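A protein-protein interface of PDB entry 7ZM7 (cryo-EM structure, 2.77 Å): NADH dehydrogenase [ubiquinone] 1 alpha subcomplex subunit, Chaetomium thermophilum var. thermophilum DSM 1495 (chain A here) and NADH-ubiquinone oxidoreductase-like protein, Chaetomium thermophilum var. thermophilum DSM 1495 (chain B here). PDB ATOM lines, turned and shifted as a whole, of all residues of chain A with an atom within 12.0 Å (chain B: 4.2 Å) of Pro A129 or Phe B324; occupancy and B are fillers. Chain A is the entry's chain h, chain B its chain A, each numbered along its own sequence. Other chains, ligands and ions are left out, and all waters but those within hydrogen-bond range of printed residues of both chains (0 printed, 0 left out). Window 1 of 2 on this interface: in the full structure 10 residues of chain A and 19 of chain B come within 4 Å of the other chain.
O of Leu B317 lies within hydrogen-bond range of N of Val B592 (2.9 Å).
NE of Arg B319 sits at hydrogen-bond distance from O of Ala B589, 2.7 Å away.
Glu A128 touches none of the printed residues of chain B.
Of the printed residues of chain B, Pro A129 touches Leu B317 and Phe B324.
Of the printed residues of chain B, Ala A131 touches Arg B319 (3.4 Å), Phe B324 (3.6 Å) and Glu B587 (3.8 Å).
Of the printed residues of chain B, Ala A132 touches Arg B319 (2.6 Å) and Glu B587 (2.8 Å).
Pro A133 touches none of the printed residues of chain B.
Printed residues of chain B within 4 Å of Arg A134: Ala B589 (3.7 Å).
Of chain A, only Trp A127 and Pro A129 come within 4 Å of Leu B317.
No residue of chain A comes within 4 Å of Val B318.
Of chain A, only Ala A131 (3.4 Å) and Ala A132 (2.6 Å) come within 4 Å of Arg B319.
No residue of chain A comes within 4 Å of Lys B323.
Of chain A, only Pro A129 and Ala A131 come within 4 Å of Phe B324.
Ala B586 touches just one residue of chain A: Trp A127 (3.5 Å).
Ala B589 touches just one residue of chain A: Arg A134 (3.7 Å).
No residue of chain A comes within 4 Å of Val B592.
The nearest printed residue of chain B that does not touch Pro A129 is Lys B323 (5.9 Å).
The nearest printed residue of chain B that does not touch Lys A130 is Phe B324 (4.2 Å).
Hydrophobic or aromatic side chains of chain B that line the printed part of chain A: Leu B317, Phe B324 and Ala B586.
Hydrophobic or aromatic side chains of chain A within 4 Å of the printed part of chain B: Trp A127, Pro A129, Ala A131 and Ala A132.
Among the printed residues, no Asp or Glu carboxylate lies within 4 Å of a Lys or Arg side-chain nitrogen of the other chain.
The backbone carbonyl oxygen (O) of Ala A132 is in hydrogen-bond range of the guanidinium group (NH1) of Arg B319 (2.6 Å).
The backbone NH (N) of Ala A132 sits at hydrogen-bond distance from the backbone carbonyl oxygen (O) of Glu B587, 2.8 Å away.
Among the printed residues, merely in contact across the chains: Trp A127 with Leu B317 (3.5 Å), Trp A127 with Ala B586 (3.5 Å), Pro A129 with Leu B317 (3.9 Å), Pro A129 with Phe B324 (3.6 Å), Lys A130 with Glu B587 (3.7 Å), Ala A131 with Arg B319 (3.4 Å), Ala A131 with Phe B324 (3.6 Å), Ala A131 with Glu B587 (3.8 Å) and Arg A134 with Ala B589 (3.7 Å).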
ATOM      1  N   GLN A 125      12.619  29.454 -18.624  1.00  0.00           N
ATOM      2  CA  GLN A 125      12.883  28.072 -18.288  1.00  0.00           C
ATOM      3  C   GLN A 125      11.664  27.488 -17.591  1.00  0.00           C
ATOM      4  O   GLN A 125      11.099  28.109 -16.692  1.00  0.00           O
ATOM      5  CB  GLN A 125      14.117  27.969 -17.401  1.00  0.00           C
ATOM      6  CG  GLN A 125      15.391  28.362 -18.102  1.00  0.00           C
ATOM      7  CD  GLN A 125      16.597  28.277 -17.196  1.00  0.00           C
ATOM      8  OE1 GLN A 125      16.473  27.983 -16.009  1.00  0.00           O
ATOM      9  NE2 GLN A 125      17.775  28.541 -17.751  1.00  0.00           N
ATOM     10  N   SER A 126      11.261  26.307 -18.022  1.00  0.00           N
ATOM     11  CA  SER A 126      10.114  25.626 -17.457  1.00  0.00           C
ATOM     12  C   SER A 126      10.553  24.613 -16.411  1.00  0.00           C
ATOM     13  O   SER A 126      11.649  24.058 -16.468  1.00  0.00           O
ATOM     14  CB  SER A 126       9.307  24.939 -18.554  1.00  0.00           C
ATOM     15  OG  SER A 126       8.186  24.292 -18.009  1.00  0.00           O
ATOM     16  N   TRP A 127       9.670  24.387 -15.447  1.00  0.00           N
ATOM     17  CA  TRP A 127       9.913  23.418 -14.394  1.00  0.00           C
ATOM     18  C   TRP A 127      10.110  22.035 -14.975  1.00  0.00           C
ATOM     19  O   TRP A 127       9.365  21.608 -15.856  1.00  0.00           O
ATOM     20  CB  TRP A 127       8.737  23.397 -13.428  1.00  0.00           C
ATOM     21  CG  TRP A 127       8.928  22.494 -12.250  1.00  0.00           C
ATOM     22  CD1 TRP A 127      10.004  22.430 -11.448  1.00  0.00           C
ATOM     23  CD2 TRP A 127       7.989  21.548 -11.744  1.00  0.00           C
ATOM     24  NE1 TRP A 127       9.808  21.506 -10.465  1.00  0.00           N
ATOM     25  CE2 TRP A 127       8.571  20.948 -10.624  1.00  0.00           C
ATOM     26  CE3 TRP A 127       6.703  21.161 -12.124  1.00  0.00           C
ATOM     27  CZ2 TRP A 127       7.921  19.971  -9.880  1.00  0.00           C
ATOM     28  CZ3 TRP A 127       6.063  20.194 -11.391  1.00  0.00           C
ATOM     29  CH2 TRP A 127       6.675  19.605 -10.284  1.00  0.00           C
ATOM     30  N   GLU A 128      11.129  21.335 -14.485  1.00  0.00           N
ATOM     31  CA  GLU A 128      11.326  19.939 -14.839  1.00  0.00           C
ATOM     32  C   GLU A 128      10.581  19.089 -13.826  1.00  0.00           C
ATOM     33  O   GLU A 128      11.071  18.920 -12.700  1.00  0.00           O
ATOM     34  CB  GLU A 128      12.796  19.582 -14.851  1.00  0.00           C
ATOM     35  CG  GLU A 128      13.099  18.308 -15.603  1.00  0.00           C
ATOM     36  CD  GLU A 128      12.562  18.321 -17.018  1.00  0.00           C
ATOM     37  OE1 GLU A 128      12.947  19.221 -17.794  1.00  0.00           O
ATOM     38  OE2 GLU A 128      11.756  17.428 -17.357  1.00  0.00           O
ATOM     39  N   PRO A 129       9.416  18.542 -14.167  1.00  0.00           N
ATOM     40  CA  PRO A 129       8.547  17.952 -13.148  1.00  0.00           C
ATOM     41  C   PRO A 129       9.228  16.847 -12.360  1.00  0.00           C
ATOM     42  O   PRO A 129       9.799  15.912 -12.920  1.00  0.00           O
ATOM     43  CB  PRO A 129       7.375  17.408 -13.967  1.00  0.00           C
ATOM     44  CG  PRO A 129       7.411  18.147 -15.216  1.00  0.00           C
ATOM     45  CD  PRO A 129       8.828  18.434 -15.506  1.00  0.00           C
ATOM     46  N   LYS A 130       9.142  16.954 -11.045  1.00  0.00           N
ATOM     47  CA  LYS A 130       9.647  15.922 -10.150  1.00  0.00           C
ATOM     48  C   LYS A 130       8.528  15.559  -9.189  1.00  0.00           C
ATOM     49  O   LYS A 130       8.204  16.336  -8.291  1.00  0.00           O
ATOM     50  CB  LYS A 130      10.884  16.394  -9.392  1.00  0.00           C
ATOM     51  CG  LYS A 130      11.385  15.403  -8.359  1.00  0.00           C
ATOM     52  CD  LYS A 130      12.671  15.891  -7.730  1.00  0.00           C
ATOM     53  CE  LYS A 130      12.434  17.159  -6.933  1.00  0.00           C
ATOM     54  NZ  LYS A 130      13.694  17.697  -6.357  1.00  0.00           N
ATOM     55  N   ALA A 131       7.941  14.387  -9.378  1.00  0.00           N
ATOM     56  CA  ALA A 131       6.878  13.928  -8.500  1.00  0.00           C
ATOM     57  C   ALA A 131       7.484  13.352  -7.229  1.00  0.00           C
ATOM     58  O   ALA A 131       8.307  12.433  -7.287  1.00  0.00           O
ATOM     59  CB  ALA A 131       6.015  12.891  -9.211  1.00  0.00           C
ATOM     60  N   ALA A 132       7.087  13.895  -6.086  1.00  0.00           N
ATOM     61  CA  ALA A 132       7.540  13.367  -4.814  1.00  0.00           C
ATOM     62  C   ALA A 132       6.970  11.968  -4.597  1.00  0.00           C
ATOM     63  O   ALA A 132       5.883  11.655  -5.084  1.00  0.00           O
ATOM     64  CB  ALA A 132       7.115  14.289  -3.676  1.00  0.00           C
ATOM     65  N   PRO A 133       7.685  11.104  -3.882  1.00  0.00           N
ATOM     66  CA  PRO A 133       7.201   9.732  -3.711  1.00  0.00           C
ATOM     67  C   PRO A 133       5.997   9.672  -2.788  1.00  0.00           C
ATOM     68  O   PRO A 133       5.812  10.518  -1.910  1.00  0.00           O
ATOM     69  CB  PRO A 133       8.400   8.992  -3.110  1.00  0.00           C
ATOM     70  CG  PRO A 133       9.362  10.039  -2.668  1.00  0.00           C
ATOM     71  CD  PRO A 133       8.855  11.390  -3.038  1.00  0.00           C
ATOM     72  N   ARG A 134       5.171   8.655  -3.004  1.00  0.00           N
ATOM     73  CA  ARG A 134       3.981   8.440  -2.191  1.00  0.00           C
ATOM     74  C   ARG A 134       4.154   7.203  -1.315  1.00  0.00           C
ATOM     75  O   ARG A 134       3.324   6.907  -0.455  1.00  0.00           O
ATOM     76  CB  ARG A 134       2.740   8.284  -3.073  1.00  0.00           C
ATOM     77  CG  ARG A 134       2.389   9.509  -3.900  1.00  0.00           C
ATOM     78  CD  ARG A 134       1.828  10.638  -3.054  1.00  0.00           C
ATOM     79  NE  ARG A 134       0.973  11.512  -3.850  1.00  0.00           N
ATOM     80  CZ  ARG A 134       0.716  12.783  -3.556  1.00  0.00           C
ATOM     81  NH1 ARG A 134      -0.075  13.502  -4.343  1.00  0.00           N
ATOM     82  NH2 ARG A 134       1.261  13.339  -2.482  1.00  0.00           N
ATOM     83  OXT ARG A 134       5.128   6.463  -1.452  1.00  0.00           O
ATOM     84  N   LEU B 317      -0.190  19.246 -15.696  1.00  0.00           N
ATOM     85  CA  LEU B 317       0.526  18.032 -15.344  1.00  0.00           C
ATOM     86  C   LEU B 317      -0.400  17.090 -14.600  1.00  0.00           C
ATOM     87  O   LEU B 317      -1.205  17.522 -13.779  1.00  0.00           O
ATOM     88  CB  LEU B 317       1.745  18.335 -14.483  1.00  0.00           C
ATOM     89  CG  LEU B 317       2.886  19.140 -15.085  1.00  0.00           C
ATOM     90  CD1 LEU B 317       3.927  19.419 -14.035  1.00  0.00           C
ATOM     91  CD2 LEU B 317       3.498  18.421 -16.259  1.00  0.00           C
ATOM     92  N   VAL B 318      -0.292  15.802 -14.900  1.00  0.00           N
ATOM     93  CA  VAL B 318      -1.035  14.757 -14.207  1.00  0.00           C
ATOM     94  C   VAL B 318      -0.026  13.732 -13.705  1.00  0.00           C
ATOM     95  O   VAL B 318       0.894  13.357 -14.436  1.00  0.00           O
ATOM     96  CB  VAL B 318      -2.072  14.088 -15.125  1.00  0.00           C
ATOM     97  CG1 VAL B 318      -2.487  12.755 -14.555  1.00  0.00           C
ATOM     98  CG2 VAL B 318      -3.263  14.976 -15.356  1.00  0.00           C
ATOM     99  N   ARG B 319      -0.166  13.314 -12.456  1.00  0.00           N
ATOM    100  CA  ARG B 319       0.717  12.305 -11.873  1.00  0.00           C
ATOM    101  C   ARG B 319       0.247  10.919 -12.293  1.00  0.00           C
ATOM    102  O   ARG B 319      -0.778  10.433 -11.812  1.00  0.00           O
ATOM    103  CB  ARG B 319       0.727  12.439 -10.357  1.00  0.00           C
ATOM    104  CG  ARG B 319       1.578  11.450  -9.648  1.00  0.00           C
ATOM    105  CD  ARG B 319       1.510  11.703  -8.169  1.00  0.00           C
ATOM    106  NE  ARG B 319       2.075  12.997  -7.825  1.00  0.00           N
ATOM    107  CZ  ARG B 319       3.196  13.150  -7.133  1.00  0.00           C
ATOM    108  NH1 ARG B 319       3.866  12.089  -6.718  1.00  0.00           N
ATOM    109  NH2 ARG B 319       3.649  14.358  -6.864  1.00  0.00           N
ATOM    110  N   LYS B 323       4.803   9.526 -11.988  1.00  0.00           N
ATOM    111  CA  LYS B 323       5.563  10.461 -12.800  1.00  0.00           C
ATOM    112  C   LYS B 323       4.609  11.495 -13.368  1.00  0.00           C
ATOM    113  O   LYS B 323       3.539  11.143 -13.868  1.00  0.00           O
ATOM    114  CB  LYS B 323       6.321   9.739 -13.921  1.00  0.00           C
ATOM    115  CG  LYS B 323       7.282  10.621 -14.710  1.00  0.00           C
ATOM    116  CD  LYS B 323       6.610  11.240 -15.919  1.00  0.00           C
ATOM    117  CE  LYS B 323       7.569  12.058 -16.749  1.00  0.00           C
ATOM    118  NZ  LYS B 323       6.880  12.690 -17.913  1.00  0.00           N
ATOM    119  N   PHE B 324       5.011  12.763 -13.317  1.00  0.00           N
ATOM    120  CA  PHE B 324       4.168  13.844 -13.809  1.00  0.00           C
ATOM    121  C   PHE B 324       4.169  13.871 -15.326  1.00  0.00           C
ATOM    122  O   PHE B 324       5.190  14.173 -15.944  1.00  0.00           O
ATOM    123  CB  PHE B 324       4.643  15.187 -13.267  1.00  0.00           C
ATOM    124  CG  PHE B 324       3.986  15.593 -12.003  1.00  0.00           C
ATOM    125  CD1 PHE B 324       2.628  15.806 -11.965  1.00  0.00           C
ATOM    126  CD2 PHE B 324       4.724  15.792 -10.859  1.00  0.00           C
ATOM    127  CE1 PHE B 324       2.015  16.184 -10.803  1.00  0.00           C
ATOM    128  CE2 PHE B 324       4.124  16.177  -9.697  1.00  0.00           C
ATOM    129  CZ  PHE B 324       2.770  16.373  -9.662  1.00  0.00           C
ATOM    130  N   GLU B 325       3.018  13.584 -15.926  1.00  0.00           N
ATOM    131  CA  GLU B 325       2.901  13.637 -17.378  1.00  0.00           C
ATOM    132  C   GLU B 325       2.241  14.929 -17.839  1.00  0.00           C
ATOM    133  O   GLU B 325       1.366  15.457 -17.156  1.00  0.00           O
ATOM    134  CB  GLU B 325       2.087  12.458 -17.903  1.00  0.00           C
ATOM    135  CG  GLU B 325       2.730  11.107 -17.763  1.00  0.00           C
ATOM    136  CD  GLU B 325       4.099  11.023 -18.405  1.00  0.00           C
ATOM    137  OE1 GLU B 325       4.424  11.867 -19.266  1.00  0.00           O
ATOM    138  OE2 GLU B 325       4.843  10.076 -18.079  1.00  0.00           O
ATOM    139  N   PRO B 326       2.668  15.462 -18.978  1.00  0.00           N
ATOM    140  CA  PRO B 326       1.950  16.586 -19.579  1.00  0.00           C
ATOM    141  C   PRO B 326       0.544  16.197 -19.985  1.00  0.00           C
ATOM    142  O   PRO B 326       0.267  15.047 -20.317  1.00  0.00           O
ATOM    143  CB  PRO B 326       2.801  16.937 -20.797  1.00  0.00           C
ATOM    144  CG  PRO B 326       4.127  16.499 -20.448  1.00  0.00           C
ATOM    145  CD  PRO B 326       4.001  15.294 -19.570  1.00  0.00           C
ATOM    146  N   ALA B 586       3.852  21.684  -6.008  1.00  0.00           N
ATOM    147  CA  ALA B 586       3.744  20.838  -7.188  1.00  0.00           C
ATOM    148  C   ALA B 586       4.374  19.470  -6.984  1.00  0.00           C
ATOM    149  O   ALA B 586       3.977  18.514  -7.648  1.00  0.00           O
ATOM    150  CB  ALA B 586       4.378  21.527  -8.392  1.00  0.00           C
ATOM    151  N   GLU B 587       5.322  19.346  -6.063  1.00  0.00           N
ATOM    152  CA  GLU B 587       5.962  18.060  -5.834  1.00  0.00           C
ATOM    153  C   GLU B 587       4.969  17.020  -5.331  1.00  0.00           C
ATOM    154  O   GLU B 587       5.092  15.833  -5.652  1.00  0.00           O
ATOM    155  CB  GLU B 587       7.108  18.226  -4.850  1.00  0.00           C
ATOM    156  CG  GLU B 587       8.317  18.906  -5.440  1.00  0.00           C
ATOM    157  CD  GLU B 587       9.223  19.501  -4.382  1.00  0.00           C
ATOM    158  OE1 GLU B 587       9.162  19.043  -3.223  1.00  0.00           O
ATOM    159  OE2 GLU B 587       9.990  20.430  -4.706  1.00  0.00           O
ATOM    160  N   ALA B 589       1.539  17.274  -5.705  1.00  0.00           N
ATOM    161  CA  ALA B 589       0.251  17.385  -6.354  1.00  0.00           C
ATOM    162  C   ALA B 589      -0.100  16.104  -7.096  1.00  0.00           C
ATOM    163  O   ALA B 589       0.762  15.317  -7.478  1.00  0.00           O
ATOM    164  CB  ALA B 589       0.251  18.566  -7.319  1.00  0.00           C
ATOM    165  N   VAL B 592      -1.293  19.379 -11.490  1.00  0.00           N
ATOM    166  CA  VAL B 592      -0.637  20.679 -11.440  1.00  0.00           C
ATOM    167  C   VAL B 592      -1.288  21.553 -12.501  1.00  0.00           C
ATOM    168  O   VAL B 592      -1.316  21.184 -13.678  1.00  0.00           O
ATOM    169  CB  VAL B 592       0.878  20.557 -11.654  1.00  0.00           C
ATOM    170  CG1 VAL B 592       1.547  21.909 -11.579  1.00  0.00           C
ATOM    171  CG2 VAL B 592       1.463  19.634 -10.631  1.00  0.00           C
